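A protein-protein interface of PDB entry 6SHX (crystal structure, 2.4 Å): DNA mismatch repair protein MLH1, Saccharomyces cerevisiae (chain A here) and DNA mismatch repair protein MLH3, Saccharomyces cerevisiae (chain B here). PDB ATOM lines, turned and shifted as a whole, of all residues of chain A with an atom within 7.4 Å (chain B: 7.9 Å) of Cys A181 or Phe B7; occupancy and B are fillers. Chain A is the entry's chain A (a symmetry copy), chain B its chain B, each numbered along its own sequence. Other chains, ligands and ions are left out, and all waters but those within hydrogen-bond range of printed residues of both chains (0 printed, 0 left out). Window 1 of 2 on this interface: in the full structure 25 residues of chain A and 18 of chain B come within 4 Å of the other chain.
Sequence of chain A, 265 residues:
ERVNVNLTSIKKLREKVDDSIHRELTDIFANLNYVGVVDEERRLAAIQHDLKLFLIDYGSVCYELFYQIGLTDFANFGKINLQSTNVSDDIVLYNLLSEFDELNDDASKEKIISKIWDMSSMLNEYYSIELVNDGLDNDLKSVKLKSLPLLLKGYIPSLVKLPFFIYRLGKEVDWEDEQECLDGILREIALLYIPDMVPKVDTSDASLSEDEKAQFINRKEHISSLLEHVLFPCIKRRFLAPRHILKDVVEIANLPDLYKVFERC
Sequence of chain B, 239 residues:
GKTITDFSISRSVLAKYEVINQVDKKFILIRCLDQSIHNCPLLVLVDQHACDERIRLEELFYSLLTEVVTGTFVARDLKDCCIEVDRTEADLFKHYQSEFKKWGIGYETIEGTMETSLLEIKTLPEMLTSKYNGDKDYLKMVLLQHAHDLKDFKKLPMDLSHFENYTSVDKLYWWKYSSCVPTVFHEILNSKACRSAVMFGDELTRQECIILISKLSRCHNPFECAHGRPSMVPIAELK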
ATOM      1  N   SER A   9      -5.145  12.893 -37.437  1.00  0.00           N
ATOM      2  CA  SER A   9      -4.095  12.276 -36.629  1.00  0.00           C
ATOM      3  C   SER A   9      -3.108  11.520 -37.517  1.00  0.00           C
ATOM      4  O   SER A   9      -1.898  11.647 -37.330  1.00  0.00           O
ATOM      5  CB  SER A   9      -4.706  11.348 -35.582  1.00  0.00           C
ATOM      6  OG  SER A   9      -5.541  10.371 -36.179  1.00  0.00           O
ATOM      7  N   LEU A  13       0.783  12.547 -38.605  1.00  0.00           N
ATOM      8  CA  LEU A  13       1.806  11.529 -38.345  1.00  0.00           C
ATOM      9  C   LEU A  13       2.637  11.261 -39.598  1.00  0.00           C
ATOM     10  O   LEU A  13       3.838  10.996 -39.497  1.00  0.00           O
ATOM     11  CB  LEU A  13       1.178  10.218 -37.843  1.00  0.00           C
ATOM     12  CG  LEU A  13       0.728  10.156 -36.381  1.00  0.00           C
ATOM     13  CD1 LEU A  13       0.119   8.809 -36.069  1.00  0.00           C
ATOM     14  CD2 LEU A  13       1.868  10.462 -35.422  1.00  0.00           C
ATOM     15  N   MET A 119     -11.357  -1.161 -27.072  1.00  0.00           N
ATOM     16  CA  MET A 119     -11.076  -0.590 -28.388  1.00  0.00           C
ATOM     17  C   MET A 119     -10.820  -1.668 -29.459  1.00  0.00           C
ATOM     18  O   MET A 119     -10.103  -1.406 -30.428  1.00  0.00           O
ATOM     19  CB  MET A 119      -9.887   0.382 -28.287  1.00  0.00           C
ATOM     20  CG  MET A 119     -10.135   1.556 -27.366  1.00  0.00           C
ATOM     21  SD  MET A 119     -10.132   3.114 -28.272  1.00  0.00           S
ATOM     22  CE  MET A 119      -9.741   4.245 -26.951  1.00  0.00           C
ATOM     23  N   MET A 122     -11.791  -0.762 -33.187  1.00  0.00           N
ATOM     24  CA  MET A 122     -10.787   0.172 -33.696  1.00  0.00           C
ATOM     25  C   MET A 122      -9.534  -0.611 -34.129  1.00  0.00           C
ATOM     26  O   MET A 122      -9.070  -0.452 -35.261  1.00  0.00           O
ATOM     27  CB  MET A 122     -10.466   1.211 -32.593  1.00  0.00           C
ATOM     28  CG  MET A 122      -9.600   2.375 -33.047  1.00  0.00           C
ATOM     29  SD  MET A 122      -7.822   2.095 -32.796  1.00  0.00           S
ATOM     30  CE  MET A 122      -7.663   2.533 -31.083  1.00  0.00           C
ATOM     31  N   LEU A 123      -9.023  -1.487 -33.237  1.00  0.00           N
ATOM     32  CA  LEU A 123      -7.847  -2.330 -33.473  1.00  0.00           C
ATOM     33  C   LEU A 123      -8.014  -3.282 -34.650  1.00  0.00           C
ATOM     34  O   LEU A 123      -7.057  -3.509 -35.385  1.00  0.00           O
ATOM     35  CB  LEU A 123      -7.462  -3.110 -32.203  1.00  0.00           C
ATOM     36  CG  LEU A 123      -6.793  -2.296 -31.101  1.00  0.00           C
ATOM     37  CD1 LEU A 123      -7.055  -2.900 -29.752  1.00  0.00           C
ATOM     38  CD2 LEU A 123      -5.305  -2.155 -31.340  1.00  0.00           C
ATOM     39  N   TYR A 126      -8.630  -0.669 -38.137  1.00  0.00           N
ATOM     40  CA  TYR A 126      -7.481   0.128 -38.537  1.00  0.00           C
ATOM     41  C   TYR A 126      -6.133  -0.599 -38.505  1.00  0.00           C
ATOM     42  O   TYR A 126      -5.209  -0.189 -39.217  1.00  0.00           O
ATOM     43  CB  TYR A 126      -7.422   1.414 -37.692  1.00  0.00           C
ATOM     44  CG  TYR A 126      -8.685   2.252 -37.749  1.00  0.00           C
ATOM     45  CD1 TYR A 126      -9.019   2.970 -38.895  1.00  0.00           C
ATOM     46  CD2 TYR A 126      -9.531   2.348 -36.651  1.00  0.00           C
ATOM     47  CE1 TYR A 126     -10.177   3.743 -38.953  1.00  0.00           C
ATOM     48  CE2 TYR A 126     -10.691   3.120 -36.693  1.00  0.00           C
ATOM     49  CZ  TYR A 126     -11.010   3.818 -37.847  1.00  0.00           C
ATOM     50  OH  TYR A 126     -12.152   4.587 -37.892  1.00  0.00           O
ATOM     51  N   TYR A 127      -6.015  -1.665 -37.691  1.00  0.00           N
ATOM     52  CA  TYR A 127      -4.752  -2.384 -37.538  1.00  0.00           C
ATOM     53  C   TYR A 127      -4.793  -3.872 -37.833  1.00  0.00           C
ATOM     54  O   TYR A 127      -3.741  -4.502 -37.792  1.00  0.00           O
ATOM     55  CB  TYR A 127      -4.193  -2.162 -36.126  1.00  0.00           C
ATOM     56  CG  TYR A 127      -3.837  -0.726 -35.840  1.00  0.00           C
ATOM     57  CD1 TYR A 127      -2.636  -0.186 -36.286  1.00  0.00           C
ATOM     58  CD2 TYR A 127      -4.700   0.098 -35.126  1.00  0.00           C
ATOM     59  CE1 TYR A 127      -2.294   1.135 -36.015  1.00  0.00           C
ATOM     60  CE2 TYR A 127      -4.370   1.422 -34.850  1.00  0.00           C
ATOM     61  CZ  TYR A 127      -3.159   1.930 -35.286  1.00  0.00           C
ATOM     62  OH  TYR A 127      -2.821   3.229 -35.042  1.00  0.00           O
ATOM     63  N   LEU A 169       0.852  -2.725 -25.113  1.00  0.00           N
ATOM     64  CA  LEU A 169      -0.372  -2.213 -25.729  1.00  0.00           C
ATOM     65  C   LEU A 169      -1.287  -1.569 -24.674  1.00  0.00           C
ATOM     66  O   LEU A 169      -1.928  -0.565 -24.965  1.00  0.00           O
ATOM     67  CB  LEU A 169      -1.102  -3.350 -26.456  1.00  0.00           C
ATOM     68  CG  LEU A 169      -1.578  -3.105 -27.887  1.00  0.00           C
ATOM     69  CD1 LEU A 169      -0.460  -2.619 -28.791  1.00  0.00           C
ATOM     70  CD2 LEU A 169      -2.155  -4.366 -28.465  1.00  0.00           C
ATOM     71  N   VAL A 173       0.786   2.314 -24.290  1.00  0.00           N
ATOM     72  CA  VAL A 173      -0.067   3.098 -25.195  1.00  0.00           C
ATOM     73  C   VAL A 173      -1.042   3.991 -24.403  1.00  0.00           C
ATOM     74  O   VAL A 173      -1.662   3.520 -23.446  1.00  0.00           O
ATOM     75  CB  VAL A 173      -0.787   2.205 -26.248  1.00  0.00           C
ATOM     76  CG1 VAL A 173      -1.691   3.018 -27.173  1.00  0.00           C
ATOM     77  CG2 VAL A 173       0.217   1.395 -27.064  1.00  0.00           C
ATOM     78  N   ASP A 174      -1.144   5.284 -24.798  1.00  0.00           N
ATOM     79  CA  ASP A 174      -2.061   6.266 -24.227  1.00  0.00           C
ATOM     80  C   ASP A 174      -3.339   6.203 -25.062  1.00  0.00           C
ATOM     81  O   ASP A 174      -3.357   6.679 -26.193  1.00  0.00           O
ATOM     82  CB  ASP A 174      -1.444   7.687 -24.236  1.00  0.00           C
ATOM     83  CG  ASP A 174      -2.380   8.844 -23.878  1.00  0.00           C
ATOM     84  OD1 ASP A 174      -3.281   8.652 -23.015  1.00  0.00           O
ATOM     85  OD2 ASP A 174      -2.198   9.945 -24.437  1.00  0.00           O
ATOM     86  N   TRP A 175      -4.397   5.591 -24.507  1.00  0.00           N
ATOM     87  CA  TRP A 175      -5.683   5.401 -25.176  1.00  0.00           C
ATOM     88  C   TRP A 175      -6.616   6.613 -25.042  1.00  0.00           C
ATOM     89  O   TRP A 175      -7.753   6.565 -25.520  1.00  0.00           O
ATOM     90  CB  TRP A 175      -6.362   4.133 -24.633  1.00  0.00           C
ATOM     91  CG  TRP A 175      -5.576   2.875 -24.857  1.00  0.00           C
ATOM     92  CD1 TRP A 175      -4.618   2.350 -24.040  1.00  0.00           C
ATOM     93  CD2 TRP A 175      -5.676   1.989 -25.982  1.00  0.00           C
ATOM     94  NE1 TRP A 175      -4.104   1.198 -24.593  1.00  0.00           N
ATOM     95  CE2 TRP A 175      -4.749   0.944 -25.777  1.00  0.00           C
ATOM     96  CE3 TRP A 175      -6.478   1.965 -27.135  1.00  0.00           C
ATOM     97  CZ2 TRP A 175      -4.605  -0.115 -26.680  1.00  0.00           C
ATOM     98  CZ3 TRP A 175      -6.308   0.934 -28.046  1.00  0.00           C
ATOM     99  CH2 TRP A 175      -5.387  -0.095 -27.812  1.00  0.00           C
ATOM    100  N   GLU A 176      -6.133   7.696 -24.410  1.00  0.00           N
ATOM    101  CA  GLU A 176      -6.908   8.907 -24.144  1.00  0.00           C
ATOM    102  C   GLU A 176      -6.702  10.029 -25.176  1.00  0.00           C
ATOM    103  O   GLU A 176      -7.300  11.098 -25.045  1.00  0.00           O
ATOM    104  CB  GLU A 176      -6.650   9.409 -22.706  1.00  0.00           C
ATOM    105  CG  GLU A 176      -6.935   8.385 -21.611  1.00  0.00           C
ATOM    106  CD  GLU A 176      -8.275   7.672 -21.677  1.00  0.00           C
ATOM    107  OE1 GLU A 176      -9.324   8.356 -21.671  1.00  0.00           O
ATOM    108  OE2 GLU A 176      -8.270   6.421 -21.740  1.00  0.00           O
ATOM    109  N   ASP A 177      -5.895   9.779 -26.213  1.00  0.00           N
ATOM    110  CA  ASP A 177      -5.650  10.743 -27.283  1.00  0.00           C
ATOM    111  C   ASP A 177      -5.504   9.993 -28.587  1.00  0.00           C
ATOM    112  O   ASP A 177      -4.705   9.058 -28.651  1.00  0.00           O
ATOM    113  CB  ASP A 177      -4.398  11.583 -27.004  1.00  0.00           C
ATOM    114  CG  ASP A 177      -4.213  12.705 -28.001  1.00  0.00           C
ATOM    115  OD1 ASP A 177      -4.783  13.794 -27.778  1.00  0.00           O
ATOM    116  OD2 ASP A 177      -3.496  12.493 -29.008  1.00  0.00           O
ATOM    117  N   GLU A 178      -6.256  10.406 -29.628  1.00  0.00           N
ATOM    118  CA  GLU A 178      -6.245   9.776 -30.950  1.00  0.00           C
ATOM    119  C   GLU A 178      -4.848   9.647 -31.558  1.00  0.00           C
ATOM    120  O   GLU A 178      -4.415   8.525 -31.806  1.00  0.00           O
ATOM    121  CB  GLU A 178      -7.203  10.487 -31.915  1.00  0.00           C
ATOM    122  CG  GLU A 178      -7.574   9.655 -33.134  1.00  0.00           C
ATOM    123  CD  GLU A 178      -8.571  10.318 -34.060  1.00  0.00           C
ATOM    124  OE1 GLU A 178      -9.706  10.586 -33.607  1.00  0.00           O
ATOM    125  OE2 GLU A 178      -8.224  10.567 -35.236  1.00  0.00           O
ATOM    126  N   GLN A 179      -4.139  10.776 -31.763  1.00  0.00           N
ATOM    127  CA  GLN A 179      -2.809  10.796 -32.372  1.00  0.00           C
ATOM    128  C   GLN A 179      -1.755  10.007 -31.584  1.00  0.00           C
ATOM    129  O   GLN A 179      -0.999   9.275 -32.201  1.00  0.00           O
ATOM    130  CB  GLN A 179      -2.344  12.233 -32.651  1.00  0.00           C
ATOM    131  CG  GLN A 179      -1.331  12.322 -33.795  1.00  0.00           C
ATOM    132  CD  GLN A 179      -0.990  13.744 -34.151  1.00  0.00           C
ATOM    133  OE1 GLN A 179      -1.841  14.524 -34.595  1.00  0.00           O
ATOM    134  NE2 GLN A 179       0.268  14.112 -33.970  1.00  0.00           N
ATOM    135  N   GLU A 180      -1.727  10.132 -30.243  1.00  0.00           N
ATOM    136  CA  GLU A 180      -0.785   9.423 -29.366  1.00  0.00           C
ATOM    137  C   GLU A 180      -1.086   7.931 -29.281  1.00  0.00           C
ATOM    138  O   GLU A 180      -0.165   7.129 -29.124  1.00  0.00           O
ATOM    139  CB  GLU A 180      -0.769  10.039 -27.952  1.00  0.00           C
ATOM    140  CG  GLU A 180      -0.256  11.469 -27.888  1.00  0.00           C
ATOM    141  CD  GLU A 180       0.961  11.770 -28.741  1.00  0.00           C
ATOM    142  OE1 GLU A 180       2.065  11.296 -28.391  1.00  0.00           O
ATOM    143  OE2 GLU A 180       0.804  12.465 -29.772  1.00  0.00           O
ATOM    144  N   CYS A 181      -2.379   7.571 -29.355  1.00  0.00           N
ATOM    145  CA  CYS A 181      -2.846   6.188 -29.319  1.00  0.00           C
ATOM    146  C   CYS A 181      -2.458   5.483 -30.594  1.00  0.00           C
ATOM    147  O   CYS A 181      -1.886   4.397 -30.528  1.00  0.00           O
ATOM    148  CB  CYS A 181      -4.355   6.123 -29.094  1.00  0.00           C
ATOM    149  SG  CYS A 181      -5.035   4.444 -29.102  1.00  0.00           S
ATOM    150  N   LEU A 182      -2.797   6.089 -31.754  1.00  0.00           N
ATOM    151  CA  LEU A 182      -2.530   5.533 -33.073  1.00  0.00           C
ATOM    152  C   LEU A 182      -1.039   5.419 -33.367  1.00  0.00           C
ATOM    153  O   LEU A 182      -0.611   4.416 -33.947  1.00  0.00           O
ATOM    154  CB  LEU A 182      -3.279   6.295 -34.186  1.00  0.00           C
ATOM    155  CG  LEU A 182      -4.817   6.403 -34.083  1.00  0.00           C
ATOM    156  CD1 LEU A 182      -5.368   7.252 -35.197  1.00  0.00           C
ATOM    157  CD2 LEU A 182      -5.500   5.046 -34.069  1.00  0.00           C
ATOM    158  N   ASP A 183      -0.250   6.421 -32.929  1.00  0.00           N
ATOM    159  CA  ASP A 183       1.207   6.466 -33.073  1.00  0.00           C
ATOM    160  C   ASP A 183       1.847   5.364 -32.208  1.00  0.00           C
ATOM    161  O   ASP A 183       2.755   4.670 -32.675  1.00  0.00           O
ATOM    162  CB  ASP A 183       1.726   7.858 -32.664  1.00  0.00           C
ATOM    163  CG  ASP A 183       3.198   8.142 -32.899  1.00  0.00           C
ATOM    164  OD1 ASP A 183       3.760   7.608 -33.883  1.00  0.00           O
ATOM    165  OD2 ASP A 183       3.781   8.925 -32.117  1.00  0.00           O
ATOM    166  N   GLY A 184       1.331   5.204 -30.983  1.00  0.00           N
ATOM    167  CA  GLY A 184       1.767   4.202 -30.015  1.00  0.00           C
ATOM    168  C   GLY A 184       1.541   2.779 -30.482  1.00  0.00           C
ATOM    169  O   GLY A 184       2.434   1.944 -30.334  1.00  0.00           O
ATOM    170  N   ILE A 185       0.344   2.495 -31.067  1.00  0.00           N
ATOM    171  CA  ILE A 185      -0.011   1.177 -31.616  1.00  0.00           C
ATOM    172  C   ILE A 185       0.944   0.840 -32.779  1.00  0.00           C
ATOM    173  O   ILE A 185       1.455  -0.283 -32.827  1.00  0.00           O
ATOM    174  CB  ILE A 185      -1.523   1.041 -31.990  1.00  0.00           C
ATOM    175  CG1 ILE A 185      -2.432   1.234 -30.755  1.00  0.00           C
ATOM    176  CG2 ILE A 185      -1.824  -0.318 -32.658  1.00  0.00           C
ATOM    177  CD1 ILE A 185      -3.943   1.419 -31.051  1.00  0.00           C
ATOM    178  N   LEU A 186       1.235   1.825 -33.668  1.00  0.00           N
ATOM    179  CA  LEU A 186       2.174   1.639 -34.783  1.00  0.00           C
ATOM    180  C   LEU A 186       3.572   1.272 -34.263  1.00  0.00           C
ATOM    181  O   LEU A 186       4.179   0.346 -34.796  1.00  0.00           O
ATOM    182  CB  LEU A 186       2.242   2.880 -35.703  1.00  0.00           C
ATOM    183  CG  LEU A 186       0.986   3.214 -36.520  1.00  0.00           C
ATOM    184  CD1 LEU A 186       1.002   4.655 -36.992  1.00  0.00           C
ATOM    185  CD2 LEU A 186       0.794   2.255 -37.673  1.00  0.00           C
ATOM    186  N   ARG A 187       4.046   1.965 -33.198  1.00  0.00           N
ATOM    187  CA  ARG A 187       5.329   1.733 -32.532  1.00  0.00           C
ATOM    188  C   ARG A 187       5.397   0.347 -31.901  1.00  0.00           C
ATOM    189  O   ARG A 187       6.459  -0.279 -31.939  1.00  0.00           O
ATOM    190  CB  ARG A 187       5.596   2.794 -31.460  1.00  0.00           C
ATOM    191  CG  ARG A 187       6.165   4.094 -31.993  1.00  0.00           C
ATOM    192  CD  ARG A 187       6.622   4.967 -30.844  1.00  0.00           C
ATOM    193  NE  ARG A 187       5.681   6.053 -30.564  1.00  0.00           N
ATOM    194  CZ  ARG A 187       4.893   6.113 -29.496  1.00  0.00           C
ATOM    195  NH1 ARG A 187       4.924   5.150 -28.583  1.00  0.00           N
ATOM    196  NH2 ARG A 187       4.072   7.139 -29.329  1.00  0.00           N
ATOM    197  N   THR B   3     -12.415  12.166 -37.241  1.00  0.00           N
ATOM    198  CA  THR B   3     -11.893  11.625 -35.985  1.00  0.00           C
ATOM    199  C   THR B   3     -12.526  10.243 -35.702  1.00  0.00           C
ATOM    200  O   THR B   3     -13.315   9.755 -36.517  1.00  0.00           O
ATOM    201  CB  THR B   3     -12.100  12.639 -34.833  1.00  0.00           C
ATOM    202  OG1 THR B   3     -13.440  13.128 -34.856  1.00  0.00           O
ATOM    203  CG2 THR B   3     -11.123  13.807 -34.886  1.00  0.00           C
ATOM    204  N   ILE B   4     -12.162   9.607 -34.566  1.00  0.00           N
ATOM    205  CA  ILE B   4     -12.703   8.310 -34.140  1.00  0.00           C
ATOM    206  C   ILE B   4     -13.647   8.540 -32.945  1.00  0.00           C
ATOM    207  O   ILE B   4     -13.237   9.099 -31.923  1.00  0.00           O
ATOM    208  CB  ILE B   4     -11.601   7.233 -33.903  1.00  0.00           C
ATOM    209  CG1 ILE B   4     -10.733   7.037 -35.174  1.00  0.00           C
ATOM    210  CG2 ILE B   4     -12.216   5.898 -33.458  1.00  0.00           C
ATOM    211  CD1 ILE B   4      -9.310   6.525 -34.940  1.00  0.00           C
ATOM    212  N   THR B   5     -14.917   8.127 -33.117  1.00  0.00           N
ATOM    213  CA  THR B   5     -16.055   8.284 -32.197  1.00  0.00           C
ATOM    214  C   THR B   5     -15.820   7.749 -30.755  1.00  0.00           C
ATOM    215  O   THR B   5     -16.271   8.397 -29.808  1.00  0.00           O
ATOM    216  CB  THR B   5     -17.342   7.681 -32.834  1.00  0.00           C
ATOM    217  OG1 THR B   5     -18.456   7.819 -31.946  1.00  0.00           O
ATOM    218  CG2 THR B   5     -17.186   6.217 -33.280  1.00  0.00           C
ATOM    219  N   ASP B   6     -15.136   6.597 -30.589  1.00  0.00           N
ATOM    220  CA  ASP B   6     -14.912   5.970 -29.274  1.00  0.00           C
ATOM    221  C   ASP B   6     -13.970   6.747 -28.326  1.00  0.00           C
ATOM    222  O   ASP B   6     -14.043   6.528 -27.112  1.00  0.00           O
ATOM    223  CB  ASP B   6     -14.447   4.502 -29.413  1.00  0.00           C
ATOM    224  CG  ASP B   6     -13.367   4.245 -30.451  1.00  0.00           C
ATOM    225  OD1 ASP B   6     -12.240   4.760 -30.277  1.00  0.00           O
ATOM    226  OD2 ASP B   6     -13.645   3.513 -31.429  1.00  0.00           O
ATOM    227  N   PHE B   7     -13.117   7.650 -28.857  1.00  0.00           N
ATOM    228  CA  PHE B   7     -12.174   8.436 -28.051  1.00  0.00           C
ATOM    229  C   PHE B   7     -12.828   9.477 -27.126  1.00  0.00           C
ATOM    230  O   PHE B   7     -12.292   9.748 -26.048  1.00  0.00           O
ATOM    231  CB  PHE B   7     -11.105   9.108 -28.933  1.00  0.00           C
ATOM    232  CG  PHE B   7     -10.008   8.181 -29.402  1.00  0.00           C
ATOM    233  CD1 PHE B   7      -8.975   7.810 -28.547  1.00  0.00           C
ATOM    234  CD2 PHE B   7      -9.999   7.690 -30.700  1.00  0.00           C
ATOM    235  CE1 PHE B   7      -7.967   6.945 -28.978  1.00  0.00           C
ATOM    236  CE2 PHE B   7      -8.985   6.831 -31.134  1.00  0.00           C
ATOM    237  CZ  PHE B   7      -7.976   6.466 -30.272  1.00  0.00           C
ATOM    238  N   SER B   8     -13.974  10.050 -27.543  1.00  0.00           N
ATOM    239  CA  SER B   8     -14.703  11.095 -26.810  1.00  0.00           C
ATOM    240  C   SER B   8     -15.699  10.594 -25.738  1.00  0.00           C
ATOM    241  O   SER B   8     -16.043  11.370 -24.838  1.00  0.00           O
ATOM    242  CB  SER B   8     -15.418  12.022 -27.790  1.00  0.00           C
ATOM    243  OG  SER B   8     -16.331  11.315 -28.613  1.00  0.00           O
ATOM    244  N   ILE B   9     -16.158   9.324 -25.837  1.00  0.00           N
ATOM    245  CA  ILE B   9     -17.150   8.709 -24.942  1.00  0.00           C
ATOM    246  C   ILE B   9     -16.666   8.624 -23.470  1.00  0.00           C
ATOM    247  O   ILE B   9     -17.463   8.893 -22.571  1.00  0.00           O
ATOM    248  CB  ILE B   9     -17.638   7.339 -25.523  1.00  0.00           C
ATOM    249  CG1 ILE B   9     -18.988   7.502 -26.254  1.00  0.00           C
ATOM    250  CG2 ILE B   9     -17.719   6.200 -24.489  1.00  0.00           C
ATOM    251  CD1 ILE B   9     -18.891   7.724 -27.762  1.00  0.00           C
ATOM    252  N   SER B  10     -15.382   8.285 -23.233  1.00  0.00           N
ATOM    253  CA  SER B  10     -14.809   8.156 -21.885  1.00  0.00           C
ATOM    254  C   SER B  10     -14.767   9.482 -21.105  1.00  0.00           C
ATOM    255  O   SER B  10     -15.138   9.505 -19.927  1.00  0.00           O
ATOM    256  CB  SER B  10     -13.424   7.521 -21.950  1.00  0.00           C
ATOM    257  OG  SER B  10     -13.490   6.212 -22.491  1.00  0.00           O
ATOM    258  N   ARG B  11     -14.336  10.578 -21.777  1.00  0.00           N
ATOM    259  CA  ARG B  11     -14.232  11.941 -21.233  1.00  0.00           C
ATOM    260  C   ARG B  11     -15.608  12.476 -20.805  1.00  0.00           C
ATOM    261  O   ARG B  11     -15.740  13.012 -19.700  1.00  0.00           O
ATOM    262  CB  ARG B  11     -13.582  12.883 -22.274  1.00  0.00           C
ATOM    263  CG  ARG B  11     -13.006  14.170 -21.683  1.00  0.00           C
ATOM    264  CD  ARG B  11     -12.426  15.085 -22.749  1.00  0.00           C
ATOM    265  NE  ARG B  11     -11.608  16.150 -22.163  1.00  0.00           N
ATOM    266  CZ  ARG B  11     -10.963  17.081 -22.860  1.00  0.00           C
ATOM    267  NH1 ARG B  11     -11.036  17.098 -24.186  1.00  0.00           N
ATOM    268  NH2 ARG B  11     -10.241  18.003 -22.238  1.00  0.00           N
ATOM    269  N   SER B  12     -16.626  12.307 -21.682  1.00  0.00           N
ATOM    270  CA  SER B  12     -18.011  12.737 -21.466  1.00  0.00           C
ATOM    271  C   SER B  12     -18.731  11.979 -20.335  1.00  0.00           C
ATOM    272  O   SER B  12     -19.677  12.526 -19.763  1.00  0.00           O
ATOM    273  CB  SER B  12     -18.808  12.668 -22.767  1.00  0.00           C
ATOM    274  OG  SER B  12     -18.722  11.392 -23.380  1.00  0.00           O
ATOM    275  N   TRP B 175       1.641  14.845 -21.478  1.00  0.00           N
ATOM    276  CA  TRP B 175       1.289  13.481 -21.872  1.00  0.00           C
ATOM    277  C   TRP B 175       1.786  13.070 -23.273  1.00  0.00           C
ATOM    278  O   TRP B 175       1.875  11.873 -23.549  1.00  0.00           O
ATOM    279  CB  TRP B 175      -0.216  13.236 -21.720  1.00  0.00           C
ATOM    280  CG  TRP B 175      -1.082  14.383 -22.142  1.00  0.00           C
ATOM    281  CD1 TRP B 175      -1.561  15.386 -21.350  1.00  0.00           C
ATOM    282  CD2 TRP B 175      -1.619  14.611 -23.449  1.00  0.00           C
ATOM    283  NE1 TRP B 175      -2.360  16.229 -22.086  1.00  0.00           N
ATOM    284  CE2 TRP B 175      -2.426  15.767 -23.375  1.00  0.00           C
ATOM    285  CE3 TRP B 175      -1.534  13.921 -24.670  1.00  0.00           C
ATOM    286  CZ2 TRP B 175      -3.121  16.263 -24.479  1.00  0.00           C
ATOM    287  CZ3 TRP B 175      -2.222  14.414 -25.764  1.00  0.00           C
ATOM    288  CH2 TRP B 175      -2.996  15.577 -25.667  1.00  0.00           C
ATOM    289  N   PHE B 223      -9.077   7.022 -15.283  1.00  0.00           N
ATOM    290  CA  PHE B 223      -9.546   5.655 -15.068  1.00  0.00           C
ATOM    291  C   PHE B 223      -8.543   4.692 -14.428  1.00  0.00           C
ATOM    292  O   PHE B 223      -8.911   3.546 -14.155  1.00  0.00           O
ATOM    293  CB  PHE B 223     -10.098   5.084 -16.375  1.00  0.00           C
ATOM    294  CG  PHE B 223     -11.106   6.018 -17.001  1.00  0.00           C
ATOM    295  CD1 PHE B 223     -12.358   6.203 -16.425  1.00  0.00           C
ATOM    296  CD2 PHE B 223     -10.782   6.759 -18.130  1.00  0.00           C
ATOM    297  CE1 PHE B 223     -13.277   7.098 -16.983  1.00  0.00           C
ATOM    298  CE2 PHE B 223     -11.704   7.645 -18.694  1.00  0.00           C
ATOM    299  CZ  PHE B 223     -12.947   7.808 -18.116  1.00  0.00           C
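The side-chain sulfur of Met A119 sits close to the side-chain carboxylate of Asp B6, 3.3 Å away.
The backbone NH of Ile B4 sits at hydrogen-bond distance from the side-chain carboxylate of Glu A178 (2.8 Å).
OG of Ser A9 sits at hydrogen-bond distance from OE2 of Glu A178 (2.9 Å).
N of Gln A179 is in hydrogen-bond range of OD2 of Asp A177, 3.3 Å away.
O of Asp A174 lies close to N of Cys A181 (3.4 Å).
OD2 of Asp A177 is in hydrogen-bond range of N of Glu A180, 3.2 Å away.
The backbone NH (N) of Glu A176 sits close to the side-chain carboxylate (OD1) of Asp A174, 3.3 Å away.
The indole nitrogen of Trp A175 lies within hydrogen-bond range of the backbone carbonyl oxygen of Leu A169, at 2.8 Å.
Among the printed residues, pairs that only touch across the chains: Asp A177 with Trp B175, Glu A178 with Thr B3, Trp A175 with Phe B7, Cys A181 with Phe B7, Glu A178 with Phe B7, Met A119 with Phe B7, Glu A176 with Phe B223, Asp A177 with Phe B7 and Tyr A126 with Ile B4.
Of the printed residues of chain B, Trp A175 touches Phe B7.
Of the printed residues of chain B, Glu A176 touches Phe B223 (3.9 Å).
Cys A181 touches just one residue of chain B: Phe B7.
Of the printed residues of chain A, Thr B3 touches Glu A178 (3.4 Å).
Printed residues of chain A within 4 Å of Ile B4: Tyr A126 (3.9 Å) and Glu A178 (2.8 Å).
Printed residues of chain A within 4 Å of Phe B7: Met A119, Trp A175, Asp A177, Glu A178 and Cys A181.
Of the printed residues of chain A, Trp B175 touches Asp A177 (3.3 Å).
Hydrophobic or aromatic side chains of chain B that line the printed part of chain A: Ile B4, Phe B7, Trp B175 and Phe B223.
Hydrophobic or aromatic side chains of chain A within 4 Å of the printed part of chain B: Met A119 and Tyr A126.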
